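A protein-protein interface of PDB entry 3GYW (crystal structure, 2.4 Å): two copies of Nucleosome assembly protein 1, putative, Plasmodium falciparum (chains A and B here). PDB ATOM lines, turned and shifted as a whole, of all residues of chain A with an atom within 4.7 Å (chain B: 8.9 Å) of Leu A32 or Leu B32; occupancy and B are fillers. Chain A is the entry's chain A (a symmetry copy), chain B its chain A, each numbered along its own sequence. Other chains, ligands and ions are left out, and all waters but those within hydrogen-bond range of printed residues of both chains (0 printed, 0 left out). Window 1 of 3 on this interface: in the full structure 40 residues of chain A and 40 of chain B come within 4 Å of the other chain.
CE1 of Phe A28 touches CD2 of Leu B35, 3.8 Å away.
Phe A28 touches Arg B36 (CZ to NH1, 3.6 Å).
Tyr B39 touches Phe A28.
Glu A31 touches Leu B35 (OE1 to CD1, 3.7 Å).
Leu B32 touches Leu A32.
Leu B35 touches Leu A32.
Leu A35 touches Phe B28.
Glu B31 touches Leu A35.
Leu B32 touches Leu A35.
Phe B28 touches Arg A36.
Phe A28 touches Leu B35, and with the chains exchanged Leu A35 touches Phe B28.
Phe A28 touches Arg B36, and with the chains exchanged Arg A36 touches Phe B28.
Leu B32 touches its own counterpart, Leu A32.
Leu A32 touches Leu B35, and with the chains exchanged Leu A35 touches Leu B32.
Positions printed for both chains: 28, 29, 30, 31, 32, 33, 34, 35 and 36.
Of the 12 pairs that touch across the chains among the printed residues, 9 have their exchanged pair printed and touching as well.
OH of Tyr B39 lies within hydrogen-bond range of OE2 of Glu A31, at 2.5 Å.
The side-chain carboxylate (OE2) of Glu A31 lies within salt-bridge range of the side-chain amino group (NZ) of Lys B38, at 2.9 Å.
Hydrophobic or aromatic side chains of chain B that line the printed part of chain A: Phe B28, Leu B32, Leu B35 and Tyr B39.
Hydrophobic or aromatic side chains of chain A within 4 Å of the printed part of chain B: Phe A28, Leu A32 and Leu A35.
Of the printed residues of chain B, Leu A32 touches Leu B32 (3.7 Å) and Leu B35 (3.6 Å).
Of chain A, only Leu A32 (3.7 Å) and Leu A35 (3.6 Å) come within 4 Å of Leu B32.
Printed residues of chain A within 4 Å of Tyr B39: Phe A28 and Glu A31.
Printed residues of chain A within 4 Å of Lys B38: Glu A31 (2.9 Å).
Printed residues of chain A within 4 Å of Glu B31: Leu A35.
Of the printed residues of chain B, Arg A36 touches Phe B28 (3.6 Å).
Tyr B24 touches none of the printed residues of chain A.
Lys B27 touches none of the printed residues of chain A.
The nearest printed residue of chain A that does not touch Leu B32 is Arg A36 (4.9 Å).
The nearest printed residue of chain A that does not touch Lys B38 is Phe A28 (7.1 Å).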
ATOM      1  N   PHE A  28       6.042   0.750 -13.914  1.00  0.00           N
ATOM      2  CA  PHE A  28       6.026   2.113 -13.386  1.00  0.00           C
ATOM      3  C   PHE A  28       4.972   2.995 -14.057  1.00  0.00           C
ATOM      4  O   PHE A  28       4.184   3.627 -13.364  1.00  0.00           O
ATOM      5  CB  PHE A  28       7.405   2.786 -13.458  1.00  0.00           C
ATOM      6  CG  PHE A  28       7.368   4.254 -13.139  1.00  0.00           C
ATOM      7  CD1 PHE A  28       7.245   4.689 -11.820  1.00  0.00           C
ATOM      8  CD2 PHE A  28       7.422   5.205 -14.160  1.00  0.00           C
ATOM      9  CE1 PHE A  28       7.193   6.049 -11.519  1.00  0.00           C
ATOM     10  CE2 PHE A  28       7.372   6.572 -13.875  1.00  0.00           C
ATOM     11  CZ  PHE A  28       7.258   6.995 -12.552  1.00  0.00           C
ATOM     12  N   GLU A  29       4.965   3.037 -15.389  1.00  0.00           N
ATOM     13  CA  GLU A  29       3.994   3.855 -16.134  1.00  0.00           C
ATOM     14  C   GLU A  29       2.548   3.415 -15.862  1.00  0.00           C
ATOM     15  O   GLU A  29       1.644   4.248 -15.742  1.00  0.00           O
ATOM     16  CB  GLU A  29       4.284   3.848 -17.642  1.00  0.00           C
ATOM     17  CG  GLU A  29       5.637   4.445 -18.059  1.00  0.00           C
ATOM     18  CD  GLU A  29       5.698   5.977 -17.991  1.00  0.00           C
ATOM     19  OE1 GLU A  29       4.644   6.632 -17.794  1.00  0.00           O
ATOM     20  OE2 GLU A  29       6.816   6.528 -18.148  1.00  0.00           O
ATOM     21  N   TYR A  30       2.351   2.104 -15.754  1.00  0.00           N
ATOM     22  CA  TYR A  30       1.058   1.528 -15.404  1.00  0.00           C
ATOM     23  C   TYR A  30       0.614   1.925 -13.992  1.00  0.00           C
ATOM     24  O   TYR A  30      -0.527   2.350 -13.793  1.00  0.00           O
ATOM     25  CB  TYR A  30       1.090   0.001 -15.556  1.00  0.00           C
ATOM     26  CG  TYR A  30      -0.168  -0.683 -15.082  1.00  0.00           C
ATOM     27  CD1 TYR A  30      -1.320  -0.695 -15.871  1.00  0.00           C
ATOM     28  CD2 TYR A  30      -0.215  -1.308 -13.837  1.00  0.00           C
ATOM     29  CE1 TYR A  30      -2.484  -1.317 -15.434  1.00  0.00           C
ATOM     30  CE2 TYR A  30      -1.379  -1.934 -13.389  1.00  0.00           C
ATOM     31  CZ  TYR A  30      -2.504  -1.935 -14.195  1.00  0.00           C
ATOM     32  OH  TYR A  30      -3.651  -2.553 -13.759  1.00  0.00           O
ATOM     33  N   GLU A  31       1.514   1.785 -13.019  1.00  0.00           N
ATOM     34  CA  GLU A  31       1.207   2.166 -11.637  1.00  0.00           C
ATOM     35  C   GLU A  31       1.029   3.679 -11.486  1.00  0.00           C
ATOM     36  O   GLU A  31       0.249   4.128 -10.655  1.00  0.00           O
ATOM     37  CB  GLU A  31       2.263   1.646 -10.658  1.00  0.00           C
ATOM     38  CG  GLU A  31       2.215   0.147 -10.409  1.00  0.00           C
ATOM     39  CD  GLU A  31       3.022  -0.253  -9.193  1.00  0.00           C
ATOM     40  OE1 GLU A  31       2.620   0.099  -8.064  1.00  0.00           O
ATOM     41  OE2 GLU A  31       4.061  -0.925  -9.354  1.00  0.00           O
ATOM     42  N   LEU A  32       1.754   4.445 -12.299  1.00  0.00           N
ATOM     43  CA  LEU A  32       1.599   5.897 -12.380  1.00  0.00           C
ATOM     44  C   LEU A  32       0.237   6.294 -12.955  1.00  0.00           C
ATOM     45  O   LEU A  32      -0.421   7.194 -12.429  1.00  0.00           O
ATOM     46  CB  LEU A  32       2.731   6.504 -13.219  1.00  0.00           C
ATOM     47  CG  LEU A  32       2.727   8.002 -13.535  1.00  0.00           C
ATOM     48  CD1 LEU A  32       2.897   8.824 -12.270  1.00  0.00           C
ATOM     49  CD2 LEU A  32       3.819   8.330 -14.532  1.00  0.00           C
ATOM     50  N   PHE A  33      -0.169   5.628 -14.038  1.00  0.00           N
ATOM     51  CA  PHE A  33      -1.491   5.837 -14.621  1.00  0.00           C
ATOM     52  C   PHE A  33      -2.591   5.563 -13.591  1.00  0.00           C
ATOM     53  O   PHE A  33      -3.537   6.339 -13.477  1.00  0.00           O
ATOM     54  CB  PHE A  33      -1.682   4.966 -15.872  1.00  0.00           C
ATOM     55  CG  PHE A  33      -2.970   5.229 -16.607  1.00  0.00           C
ATOM     56  CD1 PHE A  33      -3.074   6.296 -17.499  1.00  0.00           C
ATOM     57  CD2 PHE A  33      -4.080   4.415 -16.404  1.00  0.00           C
ATOM     58  CE1 PHE A  33      -4.267   6.548 -18.178  1.00  0.00           C
ATOM     59  CE2 PHE A  33      -5.274   4.653 -17.076  1.00  0.00           C
ATOM     60  CZ  PHE A  33      -5.370   5.723 -17.964  1.00  0.00           C
ATOM     61  N   LEU A  34      -2.450   4.463 -12.848  1.00  0.00           N
ATOM     62  CA  LEU A  34      -3.366   4.113 -11.761  1.00  0.00           C
ATOM     63  C   LEU A  34      -3.445   5.184 -10.678  1.00  0.00           C
ATOM     64  O   LEU A  34      -4.524   5.476 -10.169  1.00  0.00           O
ATOM     65  CB  LEU A  34      -2.964   2.788 -11.115  1.00  0.00           C
ATOM     66  CG  LEU A  34      -3.446   1.479 -11.738  1.00  0.00           C
ATOM     67  CD1 LEU A  34      -2.980   0.309 -10.882  1.00  0.00           C
ATOM     68  CD2 LEU A  34      -4.970   1.448 -11.907  1.00  0.00           C
ATOM     69  N   LEU A  35      -2.297   5.757 -10.326  1.00  0.00           N
ATOM     70  CA  LEU A  35      -2.235   6.781  -9.296  1.00  0.00           C
ATOM     71  C   LEU A  35      -2.932   8.062  -9.738  1.00  0.00           C
ATOM     72  O   LEU A  35      -3.714   8.630  -8.980  1.00  0.00           O
ATOM     73  CB  LEU A  35      -0.786   7.065  -8.887  1.00  0.00           C
ATOM     74  CG  LEU A  35      -0.597   7.872  -7.597  1.00  0.00           C
ATOM     75  CD1 LEU A  35      -1.089   7.088  -6.388  1.00  0.00           C
ATOM     76  CD2 LEU A  35       0.855   8.279  -7.420  1.00  0.00           C
ATOM     77  N   ARG A  36      -2.652   8.503 -10.964  1.00  0.00           N
ATOM     78  CA  ARG A  36      -3.270   9.712 -11.518  1.00  0.00           C
ATOM     79  C   ARG A  36      -4.791   9.573 -11.661  1.00  0.00           C
ATOM     80  O   ARG A  36      -5.540  10.477 -11.275  1.00  0.00           O
ATOM     81  CB  ARG A  36      -2.629  10.105 -12.854  1.00  0.00           C
ATOM     82  CG  ARG A  36      -1.144  10.448 -12.763  1.00  0.00           C
ATOM     83  CD  ARG A  36      -0.636  11.114 -14.047  1.00  0.00           C
ATOM     84  NE  ARG A  36       0.823  11.276 -14.092  1.00  0.00           N
ATOM     85  CZ  ARG A  36       1.504  12.252 -13.485  1.00  0.00           C
ATOM     86  NH1 ARG A  36       0.873  13.174 -12.755  1.00  0.00           N
ATOM     87  NH2 ARG A  36       2.831  12.306 -13.602  1.00  0.00           N
ATOM     88  N   TYR B  24      -5.695  15.989  -0.416  1.00  0.00           N
ATOM     89  CA  TYR B  24      -5.579  14.920  -1.404  1.00  0.00           C
ATOM     90  C   TYR B  24      -4.346  15.054  -2.293  1.00  0.00           C
ATOM     91  O   TYR B  24      -3.679  14.060  -2.571  1.00  0.00           O
ATOM     92  CB  TYR B  24      -6.829  14.854  -2.282  1.00  0.00           C
ATOM     93  CG  TYR B  24      -8.023  14.188  -1.638  1.00  0.00           C
ATOM     94  CD1 TYR B  24      -7.948  12.879  -1.152  1.00  0.00           C
ATOM     95  CD2 TYR B  24      -9.238  14.854  -1.542  1.00  0.00           C
ATOM     96  CE1 TYR B  24      -9.056  12.259  -0.562  1.00  0.00           C
ATOM     97  CE2 TYR B  24     -10.348  14.252  -0.959  1.00  0.00           C
ATOM     98  CZ  TYR B  24     -10.254  12.955  -0.473  1.00  0.00           C
ATOM     99  OH  TYR B  24     -11.362  12.366   0.092  1.00  0.00           O
ATOM    100  N   GLU B  25      -4.056  16.277  -2.742  1.00  0.00           N
ATOM    101  CA  GLU B  25      -2.881  16.535  -3.574  1.00  0.00           C
ATOM    102  C   GLU B  25      -1.599  16.190  -2.819  1.00  0.00           C
ATOM    103  O   GLU B  25      -0.638  15.707  -3.417  1.00  0.00           O
ATOM    104  CB  GLU B  25      -2.851  17.986  -4.063  1.00  0.00           C
ATOM    105  CG  GLU B  25      -1.779  18.271  -5.106  1.00  0.00           C
ATOM    106  CD  GLU B  25      -1.785  19.707  -5.599  1.00  0.00           C
ATOM    107  OE1 GLU B  25      -1.740  20.633  -4.763  1.00  0.00           O
ATOM    108  OE2 GLU B  25      -1.828  19.913  -6.832  1.00  0.00           O
ATOM    109  N   SER B  26      -1.604  16.424  -1.504  1.00  0.00           N
ATOM    110  CA  SER B  26      -0.495  16.037  -0.631  1.00  0.00           C
ATOM    111  C   SER B  26      -0.278  14.540  -0.667  1.00  0.00           C
ATOM    112  O   SER B  26       0.844  14.080  -0.856  1.00  0.00           O
ATOM    113  CB  SER B  26      -0.751  16.464   0.816  1.00  0.00           C
ATOM    114  OG  SER B  26      -0.151  17.712   1.084  1.00  0.00           O
ATOM    115  N   LYS B  27      -1.363  13.796  -0.472  1.00  0.00           N
ATOM    116  CA  LYS B  27      -1.329  12.341  -0.491  1.00  0.00           C
ATOM    117  C   LYS B  27      -0.851  11.837  -1.847  1.00  0.00           C
ATOM    118  O   LYS B  27      -0.074  10.886  -1.914  1.00  0.00           O
ATOM    119  CB  LYS B  27      -2.705  11.762  -0.143  1.00  0.00           C
ATOM    120  CG  LYS B  27      -2.995  11.736   1.347  1.00  0.00           C
ATOM    121  CD  LYS B  27      -4.478  11.519   1.633  1.00  0.00           C
ATOM    122  CE  LYS B  27      -4.721  11.131   3.094  1.00  0.00           C
ATOM    123  NZ  LYS B  27      -4.242  12.163   4.075  1.00  0.00           N
ATOM    124  N   PHE B  28      -1.306  12.492  -2.915  1.00  0.00           N
ATOM    125  CA  PHE B  28      -0.840  12.181  -4.264  1.00  0.00           C
ATOM    126  C   PHE B  28       0.670  12.364  -4.427  1.00  0.00           C
ATOM    127  O   PHE B  28       1.340  11.457  -4.905  1.00  0.00           O
ATOM    128  CB  PHE B  28      -1.590  12.978  -5.342  1.00  0.00           C
ATOM    129  CG  PHE B  28      -0.980  12.851  -6.710  1.00  0.00           C
ATOM    130  CD1 PHE B  28      -1.166  11.693  -7.464  1.00  0.00           C
ATOM    131  CD2 PHE B  28      -0.189  13.875  -7.233  1.00  0.00           C
ATOM    132  CE1 PHE B  28      -0.589  11.562  -8.725  1.00  0.00           C
ATOM    133  CE2 PHE B  28       0.396  13.761  -8.497  1.00  0.00           C
ATOM    134  CZ  PHE B  28       0.196  12.601  -9.245  1.00  0.00           C
ATOM    135  N   GLU B  29       1.192  13.527  -4.037  1.00  0.00           N
ATOM    136  CA  GLU B  29       2.632  13.807  -4.150  1.00  0.00           C
ATOM    137  C   GLU B  29       3.473  12.830  -3.314  1.00  0.00           C
ATOM    138  O   GLU B  29       4.544  12.390  -3.741  1.00  0.00           O
ATOM    139  CB  GLU B  29       2.960  15.259  -3.772  1.00  0.00           C
ATOM    140  CG  GLU B  29       2.324  16.335  -4.664  1.00  0.00           C
ATOM    141  CD  GLU B  29       2.979  16.481  -6.043  1.00  0.00           C
ATOM    142  OE1 GLU B  29       4.058  15.882  -6.284  1.00  0.00           O
ATOM    143  OE2 GLU B  29       2.411  17.214  -6.890  1.00  0.00           O
ATOM    144  N   TYR B  30       2.964  12.491  -2.132  1.00  0.00           N
ATOM    145  CA  TYR B  30       3.588  11.504  -1.260  1.00  0.00           C
ATOM    146  C   TYR B  30       3.605  10.107  -1.891  1.00  0.00           C
ATOM    147  O   TYR B  30       4.642   9.438  -1.899  1.00  0.00           O
ATOM    148  CB  TYR B  30       2.891  11.477   0.107  1.00  0.00           C
ATOM    149  CG  TYR B  30       3.390  10.385   1.021  1.00  0.00           C
ATOM    150  CD1 TYR B  30       4.595  10.523   1.713  1.00  0.00           C
ATOM    151  CD2 TYR B  30       2.666   9.206   1.187  1.00  0.00           C
ATOM    152  CE1 TYR B  30       5.063   9.515   2.549  1.00  0.00           C
ATOM    153  CE2 TYR B  30       3.127   8.188   2.023  1.00  0.00           C
ATOM    154  CZ  TYR B  30       4.322   8.354   2.700  1.00  0.00           C
ATOM    155  OH  TYR B  30       4.778   7.357   3.527  1.00  0.00           O
ATOM    156  N   GLU B  31       2.459   9.672  -2.414  1.00  0.00           N
ATOM    157  CA  GLU B  31       2.369   8.365  -3.072  1.00  0.00           C
ATOM    158  C   GLU B  31       3.176   8.322  -4.373  1.00  0.00           C
ATOM    159  O   GLU B  31       3.702   7.277  -4.738  1.00  0.00           O
ATOM    160  CB  GLU B  31       0.916   7.956  -3.324  1.00  0.00           C
ATOM    161  CG  GLU B  31       0.147   7.543  -2.080  1.00  0.00           C
ATOM    162  CD  GLU B  31      -1.140   6.823  -2.419  1.00  0.00           C
ATOM    163  OE1 GLU B  31      -1.073   5.688  -2.936  1.00  0.00           O
ATOM    164  OE2 GLU B  31      -2.227   7.381  -2.169  1.00  0.00           O
ATOM    165  N   LEU B  32       3.267   9.464  -5.052  1.00  0.00           N
ATOM    166  CA  LEU B  32       4.113   9.628  -6.234  1.00  0.00           C
ATOM    167  C   LEU B  32       5.601   9.525  -5.888  1.00  0.00           C
ATOM    168  O   LEU B  32       6.358   8.855  -6.595  1.00  0.00           O
ATOM    169  CB  LEU B  32       3.814  10.969  -6.916  1.00  0.00           C
ATOM    170  CG  LEU B  32       4.649  11.413  -8.120  1.00  0.00           C
ATOM    171  CD1 LEU B  32       4.434  10.486  -9.303  1.00  0.00           C
ATOM    172  CD2 LEU B  32       4.308  12.841  -8.495  1.00  0.00           C
ATOM    173  N   PHE B  33       6.011  10.199  -4.811  1.00  0.00           N
ATOM    174  CA  PHE B  33       7.380  10.101  -4.315  1.00  0.00           C
ATOM    175  C   PHE B  33       7.740   8.647  -3.994  1.00  0.00           C
ATOM    176  O   PHE B  33       8.821   8.186  -4.354  1.00  0.00           O
ATOM    177  CB  PHE B  33       7.582  11.000  -3.086  1.00  0.00           C
ATOM    178  CG  PHE B  33       9.008  11.056  -2.601  1.00  0.00           C
ATOM    179  CD1 PHE B  33       9.932  11.906  -3.208  1.00  0.00           C
ATOM    180  CD2 PHE B  33       9.428  10.257  -1.543  1.00  0.00           C
ATOM    181  CE1 PHE B  33      11.254  11.958  -2.767  1.00  0.00           C
ATOM    182  CE2 PHE B  33      10.742  10.300  -1.091  1.00  0.00           C
ATOM    183  CZ  PHE B  33      11.659  11.152  -1.705  1.00  0.00           C
ATOM    184  N   LEU B  34       6.827   7.940  -3.325  1.00  0.00           N
ATOM    185  CA  LEU B  34       6.985   6.516  -3.024  1.00  0.00           C
ATOM    186  C   LEU B  34       7.155   5.658  -4.274  1.00  0.00           C
ATOM    187  O   LEU B  34       7.963   4.733  -4.288  1.00  0.00           O
ATOM    188  CB  LEU B  34       5.792   5.993  -2.226  1.00  0.00           C
ATOM    189  CG  LEU B  34       5.784   6.156  -0.707  1.00  0.00           C
ATOM    190  CD1 LEU B  34       4.536   5.498  -0.133  1.00  0.00           C
ATOM    191  CD2 LEU B  34       7.045   5.573  -0.058  1.00  0.00           C
ATOM    192  N   LEU B  35       6.383   5.963  -5.313  1.00  0.00           N
ATOM    193  CA  LEU B  35       6.437   5.213  -6.557  1.00  0.00           C
ATOM    194  C   LEU B  35       7.768   5.413  -7.272  1.00  0.00           C
ATOM    195  O   LEU B  35       8.379   4.445  -7.718  1.00  0.00           O
ATOM    196  CB  LEU B  35       5.267   5.580  -7.475  1.00  0.00           C
ATOM    197  CG  LEU B  35       5.020   4.639  -8.659  1.00  0.00           C
ATOM    198  CD1 LEU B  35       4.587   3.260  -8.178  1.00  0.00           C
ATOM    199  CD2 LEU B  35       3.992   5.223  -9.612  1.00  0.00           C
ATOM    200  N   ARG B  36       8.212   6.665  -7.371  1.00  0.00           N
ATOM    201  CA  ARG B  36       9.487   6.992  -8.018  1.00  0.00           C
ATOM    202  C   ARG B  36      10.685   6.376  -7.284  1.00  0.00           C
ATOM    203  O   ARG B  36      11.568   5.786  -7.916  1.00  0.00           O
ATOM    204  CB  ARG B  36       9.663   8.507  -8.174  1.00  0.00           C
ATOM    205  CG  ARG B  36       8.609   9.176  -9.055  1.00  0.00           C
ATOM    206  CD  ARG B  36       9.001  10.613  -9.416  1.00  0.00           C
ATOM    207  NE  ARG B  36       7.934  11.366 -10.087  1.00  0.00           N
ATOM    208  CZ  ARG B  36       7.631  11.275 -11.384  1.00  0.00           C
ATOM    209  NH1 ARG B  36       8.301  10.442 -12.185  1.00  0.00           N
ATOM    210  NH2 ARG B  36       6.644  12.015 -11.889  1.00  0.00           N
ATOM    211  N   GLN B  37      10.701   6.495  -5.958  1.00  0.00           N
ATOM    212  CA  GLN B  37      11.741   5.865  -5.134  1.00  0.00           C
ATOM    213  C   GLN B  37      11.780   4.343  -5.285  1.00  0.00           C
ATOM    214  O   GLN B  37      12.858   3.771  -5.469  1.00  0.00           O
ATOM    215  CB  GLN B  37      11.607   6.258  -3.654  1.00  0.00           C
ATOM    216  CG  GLN B  37      11.954   7.719  -3.354  1.00  0.00           C
ATOM    217  CD  GLN B  37      13.368   8.099  -3.772  1.00  0.00           C
ATOM    218  OE1 GLN B  37      13.568   8.786  -4.781  1.00  0.00           O
ATOM    219  NE2 GLN B  37      14.357   7.642  -3.005  1.00  0.00           N
ATOM    220  N   LYS B  38      10.612   3.698  -5.212  1.00  0.00           N
ATOM    221  CA  LYS B  38      10.496   2.246  -5.396  1.00  0.00           C
ATOM    222  C   LYS B  38      11.140   1.775  -6.700  1.00  0.00           C
ATOM    223  O   LYS B  38      11.872   0.785  -6.717  1.00  0.00           O
ATOM    224  CB  LYS B  38       9.027   1.807  -5.345  1.00  0.00           C
ATOM    225  CG  LYS B  38       8.774   0.329  -5.649  1.00  0.00           C
ATOM    226  CD  LYS B  38       7.279   0.047  -5.771  1.00  0.00           C
ATOM    227  CE  LYS B  38       7.010  -1.291  -6.461  1.00  0.00           C
ATOM    228  NZ  LYS B  38       5.612  -1.381  -7.002  1.00  0.00           N
ATOM    229  N   TYR B  39      10.871   2.498  -7.784  1.00  0.00           N
ATOM    230  CA  TYR B  39      11.406   2.135  -9.090  1.00  0.00           C
ATOM    231  C   TYR B  39      12.864   2.548  -9.341  1.00  0.00           C
ATOM    232  O   TYR B  39      13.555   1.901 -10.124  1.00  0.00           O
ATOM    233  CB  TYR B  39      10.446   2.554 -10.211  1.00  0.00           C
ATOM    234  CG  TYR B  39       9.313   1.565 -10.329  1.00  0.00           C
ATOM    235  CD1 TYR B  39       9.449   0.414 -11.109  1.00  0.00           C
ATOM    236  CD2 TYR B  39       8.127   1.743  -9.615  1.00  0.00           C
ATOM    237  CE1 TYR B  39       8.427  -0.515 -11.196  1.00  0.00           C
ATOM    238  CE2 TYR B  39       7.097   0.819  -9.698  1.00  0.00           C
ATOM    239  CZ  TYR B  39       7.254  -0.307 -10.489  1.00  0.00           C
ATOM    240  OH  TYR B  39       6.244  -1.233 -10.573  1.00  0.00           O
ATOM    241  N   TYR B 103      19.595  10.619  -6.056  1.00  0.00           N
ATOM    242  CA  TYR B 103      18.845  11.746  -5.492  1.00  0.00           C
ATOM    243  C   TYR B 103      19.473  12.262  -4.199  1.00  0.00           C
ATOM    244  O   TYR B 103      20.614  11.927  -3.865  1.00  0.00           O
ATOM    245  CB  TYR B 103      17.383  11.370  -5.244  1.00  0.00           C
ATOM    246  CG  TYR B 103      16.604  10.971  -6.486  1.00  0.00           C
ATOM    247  CD1 TYR B 103      16.305  11.904  -7.484  1.00  0.00           C
ATOM    248  CD2 TYR B 103      16.148   9.660  -6.652  1.00  0.00           C
ATOM    249  CE1 TYR B 103      15.582  11.535  -8.624  1.00  0.00           C
ATOM    250  CE2 TYR B 103      15.421   9.281  -7.786  1.00  0.00           C
ATOM    251  CZ  TYR B 103      15.143  10.221  -8.764  1.00  0.00           C
ATOM    252  OH  TYR B 103      14.424   9.842  -9.879  1.00  0.00           O
